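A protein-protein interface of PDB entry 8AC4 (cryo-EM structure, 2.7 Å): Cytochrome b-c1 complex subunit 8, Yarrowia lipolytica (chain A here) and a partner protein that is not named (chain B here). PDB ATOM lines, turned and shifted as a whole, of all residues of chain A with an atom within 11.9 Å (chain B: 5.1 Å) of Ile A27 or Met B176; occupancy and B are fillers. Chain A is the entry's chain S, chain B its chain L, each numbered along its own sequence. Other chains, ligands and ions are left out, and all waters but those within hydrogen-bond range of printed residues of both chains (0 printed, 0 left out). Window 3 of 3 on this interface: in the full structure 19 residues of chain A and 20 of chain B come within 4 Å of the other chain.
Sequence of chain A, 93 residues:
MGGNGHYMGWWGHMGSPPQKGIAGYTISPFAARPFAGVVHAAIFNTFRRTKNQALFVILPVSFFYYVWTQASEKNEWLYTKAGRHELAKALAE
Hydrophobic or aromatic side chains of chain A that line the printed part of chain B: Ile A27. Among the printed residues, 7 pairs touch across the chains. Among the printed residues, no Asp or Glu carboxylate lies within 4 Å of a Lys or Arg side-chain nitrogen of the other chain.
The backbone carbonyl oxygen (O) of Met B176 lies within hydrogen-bond range of the side-chain amide nitrogen (NE2) of Gln B178 (2.9 Å). N of Phe A30 lies close to OG of Ser A28. The side-chain hydroxyl (OG) of Ser B266 sits at hydrogen-bond distance from the backbone carbonyl oxygen (O) of Val B264 (2.8 Å). OG1 of Thr B173 sits at hydrogen-bond distance from OG of Ser B266.
Among the printed residues, merely in contact across the chains: Gly A24 with Glu B267 (3.7 Å), Tyr A25 with Glu B267 (3.4 Å), Thr A26 with Ser B266 (3.2 Å), Ile A27 with Met B176 (3.7 Å) and Ile A27 with Gly B265 (3.6 Å).
Ile A27 touches two residues of chain B. Of chain A, only Ile A27 comes within 4 Å of Met B176. No residue of chain A comes within 4 Å of Thr B173. No residue of chain A comes within 4 Å of Ala B174. No residue of chain A comes within 4 Å of Asn B177. Gln B178 touches none of the printed residues of chain A. No residue of chain A comes within 4 Å of Val B264. Gly B265 touches two residues of chain A. Of chain A, only Gly A24 (3.7 Å), Tyr A25 (3.4 Å) and Thr A26 (3.0 Å) come within 4 Å of Glu B267. Of the printed residues of chain B, Thr A26 touches Ser B266 and Glu B267. Printed residues of chain B within 4 Å of Ser A28: Gly B265 (2.8 Å). Printed residues of chain B within 4 Å of Gly A24: Glu B267. Of the printed residues of chain B, Tyr A25 touches Glu B267 (3.4 Å). Arg A33 touches none of the printed residues of chain B. The nearest residue of chain A that does not touch Met B176 is Thr A26 (5.2 Å).
O of Thr A26 sits at hydrogen-bond distance from N of Glu B267. The backbone NH (N) of Ser A28 is in hydrogen-bond range of the backbone carbonyl oxygen (O) of Gly B265.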
ATOM      1  N   ALA A  23     -16.969 -33.030  35.352  1.00  0.00           N
ATOM      2  CA  ALA A  23     -17.835 -32.975  34.185  1.00  0.00           C
ATOM      3  C   ALA A  23     -17.048 -32.320  33.060  1.00  0.00           C
ATOM      4  O   ALA A  23     -16.452 -31.270  33.279  1.00  0.00           O
ATOM      5  CB  ALA A  23     -19.082 -32.190  34.504  1.00  0.00           C
ATOM      6  N   GLY A  24     -17.020 -32.947  31.884  1.00  0.00           N
ATOM      7  CA  GLY A  24     -16.308 -32.367  30.759  1.00  0.00           C
ATOM      8  C   GLY A  24     -17.297 -31.924  29.694  1.00  0.00           C
ATOM      9  O   GLY A  24     -18.274 -32.616  29.444  1.00  0.00           O
ATOM     10  N   TYR A  25     -17.036 -30.786  29.066  1.00  0.00           N
ATOM     11  CA  TYR A  25     -17.966 -30.298  28.071  1.00  0.00           C
ATOM     12  C   TYR A  25     -17.202 -29.868  26.844  1.00  0.00           C
ATOM     13  O   TYR A  25     -16.140 -29.273  26.967  1.00  0.00           O
ATOM     14  CB  TYR A  25     -18.606 -29.015  28.572  1.00  0.00           C
ATOM     15  CG  TYR A  25     -19.371 -29.242  29.837  1.00  0.00           C
ATOM     16  CD1 TYR A  25     -18.722 -29.293  31.064  1.00  0.00           C
ATOM     17  CD2 TYR A  25     -20.745 -29.417  29.800  1.00  0.00           C
ATOM     18  CE1 TYR A  25     -19.431 -29.499  32.233  1.00  0.00           C
ATOM     19  CE2 TYR A  25     -21.469 -29.640  30.958  1.00  0.00           C
ATOM     20  CZ  TYR A  25     -20.807 -29.672  32.171  1.00  0.00           C
ATOM     21  OH  TYR A  25     -21.530 -29.880  33.300  1.00  0.00           O
ATOM     22  N   THR A  26     -17.762 -30.135  25.666  1.00  0.00           N
ATOM     23  CA  THR A  26     -17.161 -29.570  24.474  1.00  0.00           C
ATOM     24  C   THR A  26     -18.176 -29.427  23.352  1.00  0.00           C
ATOM     25  O   THR A  26     -19.243 -30.013  23.397  1.00  0.00           O
ATOM     26  CB  THR A  26     -15.947 -30.382  24.023  1.00  0.00           C
ATOM     27  OG1 THR A  26     -15.304 -29.514  23.088  1.00  0.00           O
ATOM     28  CG2 THR A  26     -16.321 -31.704  23.397  1.00  0.00           C
ATOM     29  N   ILE A  27     -17.814 -28.681  22.316  1.00  0.00           N
ATOM     30  CA  ILE A  27     -18.732 -28.528  21.203  1.00  0.00           C
ATOM     31  C   ILE A  27     -18.120 -29.111  19.935  1.00  0.00           C
ATOM     32  O   ILE A  27     -16.902 -29.222  19.811  1.00  0.00           O
ATOM     33  CB  ILE A  27     -19.142 -27.056  21.049  1.00  0.00           C
ATOM     34  CG1 ILE A  27     -17.910 -26.186  20.790  1.00  0.00           C
ATOM     35  CG2 ILE A  27     -19.929 -26.610  22.277  1.00  0.00           C
ATOM     36  CD1 ILE A  27     -18.220 -24.777  20.359  1.00  0.00           C
ATOM     37  N   SER A  28     -19.000 -29.455  18.991  1.00  0.00           N
ATOM     38  CA  SER A  28     -18.680 -30.025  17.693  1.00  0.00           C
ATOM     39  C   SER A  28     -17.698 -29.150  16.917  1.00  0.00           C
ATOM     40  O   SER A  28     -17.768 -27.926  16.975  1.00  0.00           O
ATOM     41  CB  SER A  28     -19.952 -30.137  16.922  1.00  0.00           C
ATOM     42  OG  SER A  28     -19.693 -30.555  15.598  1.00  0.00           O
ATOM     43  N   PRO A  29     -16.789 -29.738  16.115  1.00  0.00           N
ATOM     44  CA  PRO A  29     -15.955 -28.946  15.216  1.00  0.00           C
ATOM     45  C   PRO A  29     -16.776 -28.092  14.264  1.00  0.00           C
ATOM     46  O   PRO A  29     -16.345 -27.002  13.923  1.00  0.00           O
ATOM     47  CB  PRO A  29     -15.130 -29.971  14.434  1.00  0.00           C
ATOM     48  CG  PRO A  29     -15.844 -31.282  14.671  1.00  0.00           C
ATOM     49  CD  PRO A  29     -16.490 -31.172  16.036  1.00  0.00           C
ATOM     50  N   PHE A  30     -17.942 -28.588  13.844  1.00  0.00           N
ATOM     51  CA  PHE A  30     -18.761 -27.809  12.929  1.00  0.00           C
ATOM     52  C   PHE A  30     -19.499 -26.674  13.625  1.00  0.00           C
ATOM     53  O   PHE A  30     -19.979 -25.763  12.956  1.00  0.00           O
ATOM     54  CB  PHE A  30     -19.791 -28.669  12.209  1.00  0.00           C
ATOM     55  CG  PHE A  30     -19.176 -29.677  11.281  1.00  0.00           C
ATOM     56  CD1 PHE A  30     -19.064 -29.408   9.924  1.00  0.00           C
ATOM     57  CD2 PHE A  30     -18.715 -30.901  11.759  1.00  0.00           C
ATOM     58  CE1 PHE A  30     -18.502 -30.340   9.062  1.00  0.00           C
ATOM     59  CE2 PHE A  30     -18.143 -31.827  10.898  1.00  0.00           C
ATOM     60  CZ  PHE A  30     -18.041 -31.547   9.549  1.00  0.00           C
ATOM     61  N   ALA A  31     -19.587 -26.717  14.955  1.00  0.00           N
ATOM     62  CA  ALA A  31     -20.266 -25.642  15.659  1.00  0.00           C
ATOM     63  C   ALA A  31     -19.281 -24.547  16.067  1.00  0.00           C
ATOM     64  O   ALA A  31     -19.693 -23.467  16.485  1.00  0.00           O
ATOM     65  CB  ALA A  31     -20.955 -26.218  16.861  1.00  0.00           C
ATOM     66  N   ALA A  32     -17.982 -24.840  15.991  1.00  0.00           N
ATOM     67  CA  ALA A  32     -17.002 -23.917  16.533  1.00  0.00           C
ATOM     68  C   ALA A  32     -16.334 -23.134  15.412  1.00  0.00           C
ATOM     69  O   ALA A  32     -16.216 -23.607  14.284  1.00  0.00           O
ATOM     70  CB  ALA A  32     -15.986 -24.655  17.356  1.00  0.00           C
ATOM     71  N   ARG A  33     -15.868 -21.940  15.763  1.00  0.00           N
ATOM     72  CA  ARG A  33     -14.996 -21.204  14.876  1.00  0.00           C
ATOM     73  C   ARG A  33     -13.567 -21.687  15.114  1.00  0.00           C
ATOM     74  O   ARG A  33     -12.989 -21.425  16.162  1.00  0.00           O
ATOM     75  CB  ARG A  33     -15.209 -19.715  15.135  1.00  0.00           C
ATOM     76  CG  ARG A  33     -16.587 -19.213  14.734  1.00  0.00           C
ATOM     77  CD  ARG A  33     -16.627 -17.700  14.819  1.00  0.00           C
ATOM     78  NE  ARG A  33     -16.646 -17.272  16.210  1.00  0.00           N
ATOM     79  CZ  ARG A  33     -17.746 -16.986  16.899  1.00  0.00           C
ATOM     80  NH1 ARG A  33     -18.936 -17.052  16.323  1.00  0.00           N
ATOM     81  NH2 ARG A  33     -17.652 -16.615  18.163  1.00  0.00           N
ATOM     82  N   PRO A  34     -12.924 -22.400  14.163  1.00  0.00           N
ATOM     83  CA  PRO A  34     -11.620 -23.005  14.429  1.00  0.00           C
ATOM     84  C   PRO A  34     -10.546 -21.948  14.667  1.00  0.00           C
ATOM     85  O   PRO A  34      -9.596 -22.194  15.405  1.00  0.00           O
ATOM     86  CB  PRO A  34     -11.264 -23.767  13.151  1.00  0.00           C
ATOM     87  CG  PRO A  34     -12.521 -23.756  12.325  1.00  0.00           C
ATOM     88  CD  PRO A  34     -13.346 -22.571  12.770  1.00  0.00           C
ATOM     89  N   PHE A  35     -10.726 -20.761  14.073  1.00  0.00           N
ATOM     90  CA  PHE A  35      -9.745 -19.698  14.198  1.00  0.00           C
ATOM     91  C   PHE A  35     -10.222 -18.597  15.127  1.00  0.00           C
ATOM     92  O   PHE A  35      -9.750 -17.468  15.016  1.00  0.00           O
ATOM     93  CB  PHE A  35      -9.436 -19.095  12.830  1.00  0.00           C
ATOM     94  CG  PHE A  35      -8.520 -19.964  12.020  1.00  0.00           C
ATOM     95  CD1 PHE A  35      -9.032 -20.921  11.158  1.00  0.00           C
ATOM     96  CD2 PHE A  35      -7.144 -19.855  12.146  1.00  0.00           C
ATOM     97  CE1 PHE A  35      -8.183 -21.738  10.422  1.00  0.00           C
ATOM     98  CE2 PHE A  35      -6.297 -20.663  11.402  1.00  0.00           C
ATOM     99  CZ  PHE A  35      -6.816 -21.608  10.546  1.00  0.00           C
ATOM    100  N   ALA A  36     -11.136 -18.917  16.042  1.00  0.00           N
ATOM    101  CA  ALA A  36     -11.569 -17.930  17.015  1.00  0.00           C
ATOM    102  C   ALA A  36     -10.368 -17.475  17.838  1.00  0.00           C
ATOM    103  O   ALA A  36      -9.583 -18.306  18.291  1.00  0.00           O
ATOM    104  CB  ALA A  36     -12.644 -18.505  17.897  1.00  0.00           C
ATOM    105  N   HIS B 171     -30.620 -32.308  27.287  1.00  0.00           N
ATOM    106  CA  HIS B 171     -31.282 -31.073  26.892  1.00  0.00           C
ATOM    107  C   HIS B 171     -30.385 -29.864  27.111  1.00  0.00           C
ATOM    108  O   HIS B 171     -30.401 -28.929  26.317  1.00  0.00           O
ATOM    109  CB  HIS B 171     -32.558 -30.875  27.683  1.00  0.00           C
ATOM    110  CG  HIS B 171     -33.673 -31.702  27.170  1.00  0.00           C
ATOM    111  ND1 HIS B 171     -33.734 -33.057  27.407  1.00  0.00           N
ATOM    112  CD2 HIS B 171     -34.757 -31.380  26.436  1.00  0.00           C
ATOM    113  CE1 HIS B 171     -34.803 -33.550  26.829  1.00  0.00           C
ATOM    114  NE2 HIS B 171     -35.450 -32.539  26.229  1.00  0.00           N
ATOM    115  N   ALA B 172     -29.643 -29.871  28.220  1.00  0.00           N
ATOM    116  CA  ALA B 172     -28.827 -28.729  28.592  1.00  0.00           C
ATOM    117  C   ALA B 172     -27.793 -28.456  27.509  1.00  0.00           C
ATOM    118  O   ALA B 172     -27.554 -27.300  27.173  1.00  0.00           O
ATOM    119  CB  ALA B 172     -28.159 -28.993  29.912  1.00  0.00           C
ATOM    120  N   THR B 173     -27.200 -29.520  26.962  1.00  0.00           N
ATOM    121  CA  THR B 173     -26.149 -29.337  25.980  1.00  0.00           C
ATOM    122  C   THR B 173     -26.712 -29.144  24.573  1.00  0.00           C
ATOM    123  O   THR B 173     -26.255 -28.256  23.864  1.00  0.00           O
ATOM    124  CB  THR B 173     -25.084 -30.424  26.083  1.00  0.00           C
ATOM    125  OG1 THR B 173     -23.957 -29.871  25.411  1.00  0.00           O
ATOM    126  CG2 THR B 173     -25.467 -31.732  25.429  1.00  0.00           C
ATOM    127  N   ALA B 174     -27.712 -29.944  24.182  1.00  0.00           N
ATOM    128  CA  ALA B 174     -28.331 -29.810  22.870  1.00  0.00           C
ATOM    129  C   ALA B 174     -28.888 -28.406  22.664  1.00  0.00           C
ATOM    130  O   ALA B 174     -28.787 -27.868  21.568  1.00  0.00           O
ATOM    131  CB  ALA B 174     -29.403 -30.847  22.658  1.00  0.00           C
ATOM    132  N   PHE B 175     -29.503 -27.823  23.697  1.00  0.00           N
ATOM    133  CA  PHE B 175     -30.108 -26.519  23.501  1.00  0.00           C
ATOM    134  C   PHE B 175     -29.416 -25.539  24.413  1.00  0.00           C
ATOM    135  O   PHE B 175     -30.058 -24.909  25.233  1.00  0.00           O
ATOM    136  CB  PHE B 175     -31.608 -26.557  23.778  1.00  0.00           C
ATOM    137  CG  PHE B 175     -32.311 -27.492  22.842  1.00  0.00           C
ATOM    138  CD1 PHE B 175     -32.403 -27.205  21.484  1.00  0.00           C
ATOM    139  CD2 PHE B 175     -32.837 -28.686  23.313  1.00  0.00           C
ATOM    140  CE1 PHE B 175     -33.034 -28.089  20.618  1.00  0.00           C
ATOM    141  CE2 PHE B 175     -33.480 -29.560  22.451  1.00  0.00           C
ATOM    142  CZ  PHE B 175     -33.570 -29.263  21.107  1.00  0.00           C
ATOM    143  N   MET B 176     -28.099 -25.469  24.269  1.00  0.00           N
ATOM    144  CA  MET B 176     -27.225 -24.708  25.134  1.00  0.00           C
ATOM    145  C   MET B 176     -27.701 -23.257  25.217  1.00  0.00           C
ATOM    146  O   MET B 176     -27.951 -22.642  24.187  1.00  0.00           O
ATOM    147  CB  MET B 176     -25.862 -24.734  24.463  1.00  0.00           C
ATOM    148  CG  MET B 176     -24.733 -24.696  25.404  1.00  0.00           C
ATOM    149  SD  MET B 176     -23.286 -24.845  24.351  1.00  0.00           S
ATOM    150  CE  MET B 176     -22.990 -26.610  24.418  1.00  0.00           C
ATOM    151  N   ASN B 177     -27.853 -22.746  26.447  1.00  0.00           N
ATOM    152  CA  ASN B 177     -28.294 -21.389  26.777  1.00  0.00           C
ATOM    153  C   ASN B 177     -29.623 -20.997  26.131  1.00  0.00           C
ATOM    154  O   ASN B 177     -29.862 -19.827  25.837  1.00  0.00           O
ATOM    155  CB  ASN B 177     -27.259 -20.318  26.436  1.00  0.00           C
ATOM    156  CG  ASN B 177     -25.856 -20.724  26.820  1.00  0.00           C
ATOM    157  OD1 ASN B 177     -25.580 -21.015  27.982  1.00  0.00           O
ATOM    158  ND2 ASN B 177     -24.972 -20.765  25.839  1.00  0.00           N
ATOM    159  N   GLN B 178     -30.501 -21.967  25.919  1.00  0.00           N
ATOM    160  CA  GLN B 178     -31.813 -21.649  25.395  1.00  0.00           C
ATOM    161  C   GLN B 178     -32.852 -22.143  26.396  1.00  0.00           C
ATOM    162  O   GLN B 178     -32.552 -23.025  27.188  1.00  0.00           O
ATOM    163  CB  GLN B 178     -31.975 -22.300  24.026  1.00  0.00           C
ATOM    164  CG  GLN B 178     -31.040 -21.725  22.977  1.00  0.00           C
ATOM    165  CD  GLN B 178     -30.797 -22.711  21.862  1.00  0.00           C
ATOM    166  OE1 GLN B 178     -31.659 -22.949  21.022  1.00  0.00           O
ATOM    167  NE2 GLN B 178     -29.610 -23.293  21.847  1.00  0.00           N
ATOM    168  N   VAL B 264     -27.106 -27.513  19.386  1.00  0.00           N
ATOM    169  CA  VAL B 264     -25.658 -27.412  19.426  1.00  0.00           C
ATOM    170  C   VAL B 264     -25.082 -28.816  19.507  1.00  0.00           C
ATOM    171  O   VAL B 264     -25.275 -29.497  20.503  1.00  0.00           O
ATOM    172  CB  VAL B 264     -25.159 -26.607  20.636  1.00  0.00           C
ATOM    173  CG1 VAL B 264     -23.645 -26.556  20.642  1.00  0.00           C
ATOM    174  CG2 VAL B 264     -25.743 -25.209  20.713  1.00  0.00           C
ATOM    175  N   GLY B 265     -24.339 -29.235  18.480  1.00  0.00           N
ATOM    176  CA  GLY B 265     -23.672 -30.521  18.583  1.00  0.00           C
ATOM    177  C   GLY B 265     -22.573 -30.437  19.630  1.00  0.00           C
ATOM    178  O   GLY B 265     -21.759 -29.521  19.591  1.00  0.00           O
ATOM    179  N   SER B 266     -22.580 -31.359  20.587  1.00  0.00           N
ATOM    180  CA  SER B 266     -21.771 -31.137  21.768  1.00  0.00           C
ATOM    181  C   SER B 266     -21.760 -32.399  22.615  1.00  0.00           C
ATOM    182  O   SER B 266     -22.503 -33.324  22.327  1.00  0.00           O
ATOM    183  CB  SER B 266     -22.320 -29.962  22.537  1.00  0.00           C
ATOM    184  OG  SER B 266     -23.719 -30.096  22.727  1.00  0.00           O
ATOM    185  N   GLU B 267     -20.902 -32.462  23.628  1.00  0.00           N
ATOM    186  CA  GLU B 267     -20.957 -33.612  24.511  1.00  0.00           C
ATOM    187  C   GLU B 267     -20.738 -33.185  25.943  1.00  0.00           C
ATOM    188  O   GLU B 267     -20.069 -32.188  26.203  1.00  0.00           O
ATOM    189  CB  GLU B 267     -19.935 -34.696  24.208  1.00  0.00           C
ATOM    190  CG  GLU B 267     -18.676 -34.106  23.694  1.00  0.00           C
ATOM    191  CD  GLU B 267     -17.538 -35.101  23.754  1.00  0.00           C
ATOM    192  OE1 GLU B 267     -17.611 -36.130  23.046  1.00  0.00           O
ATOM    193  OE2 GLU B 267     -16.577 -34.846  24.507  1.00  0.00           O
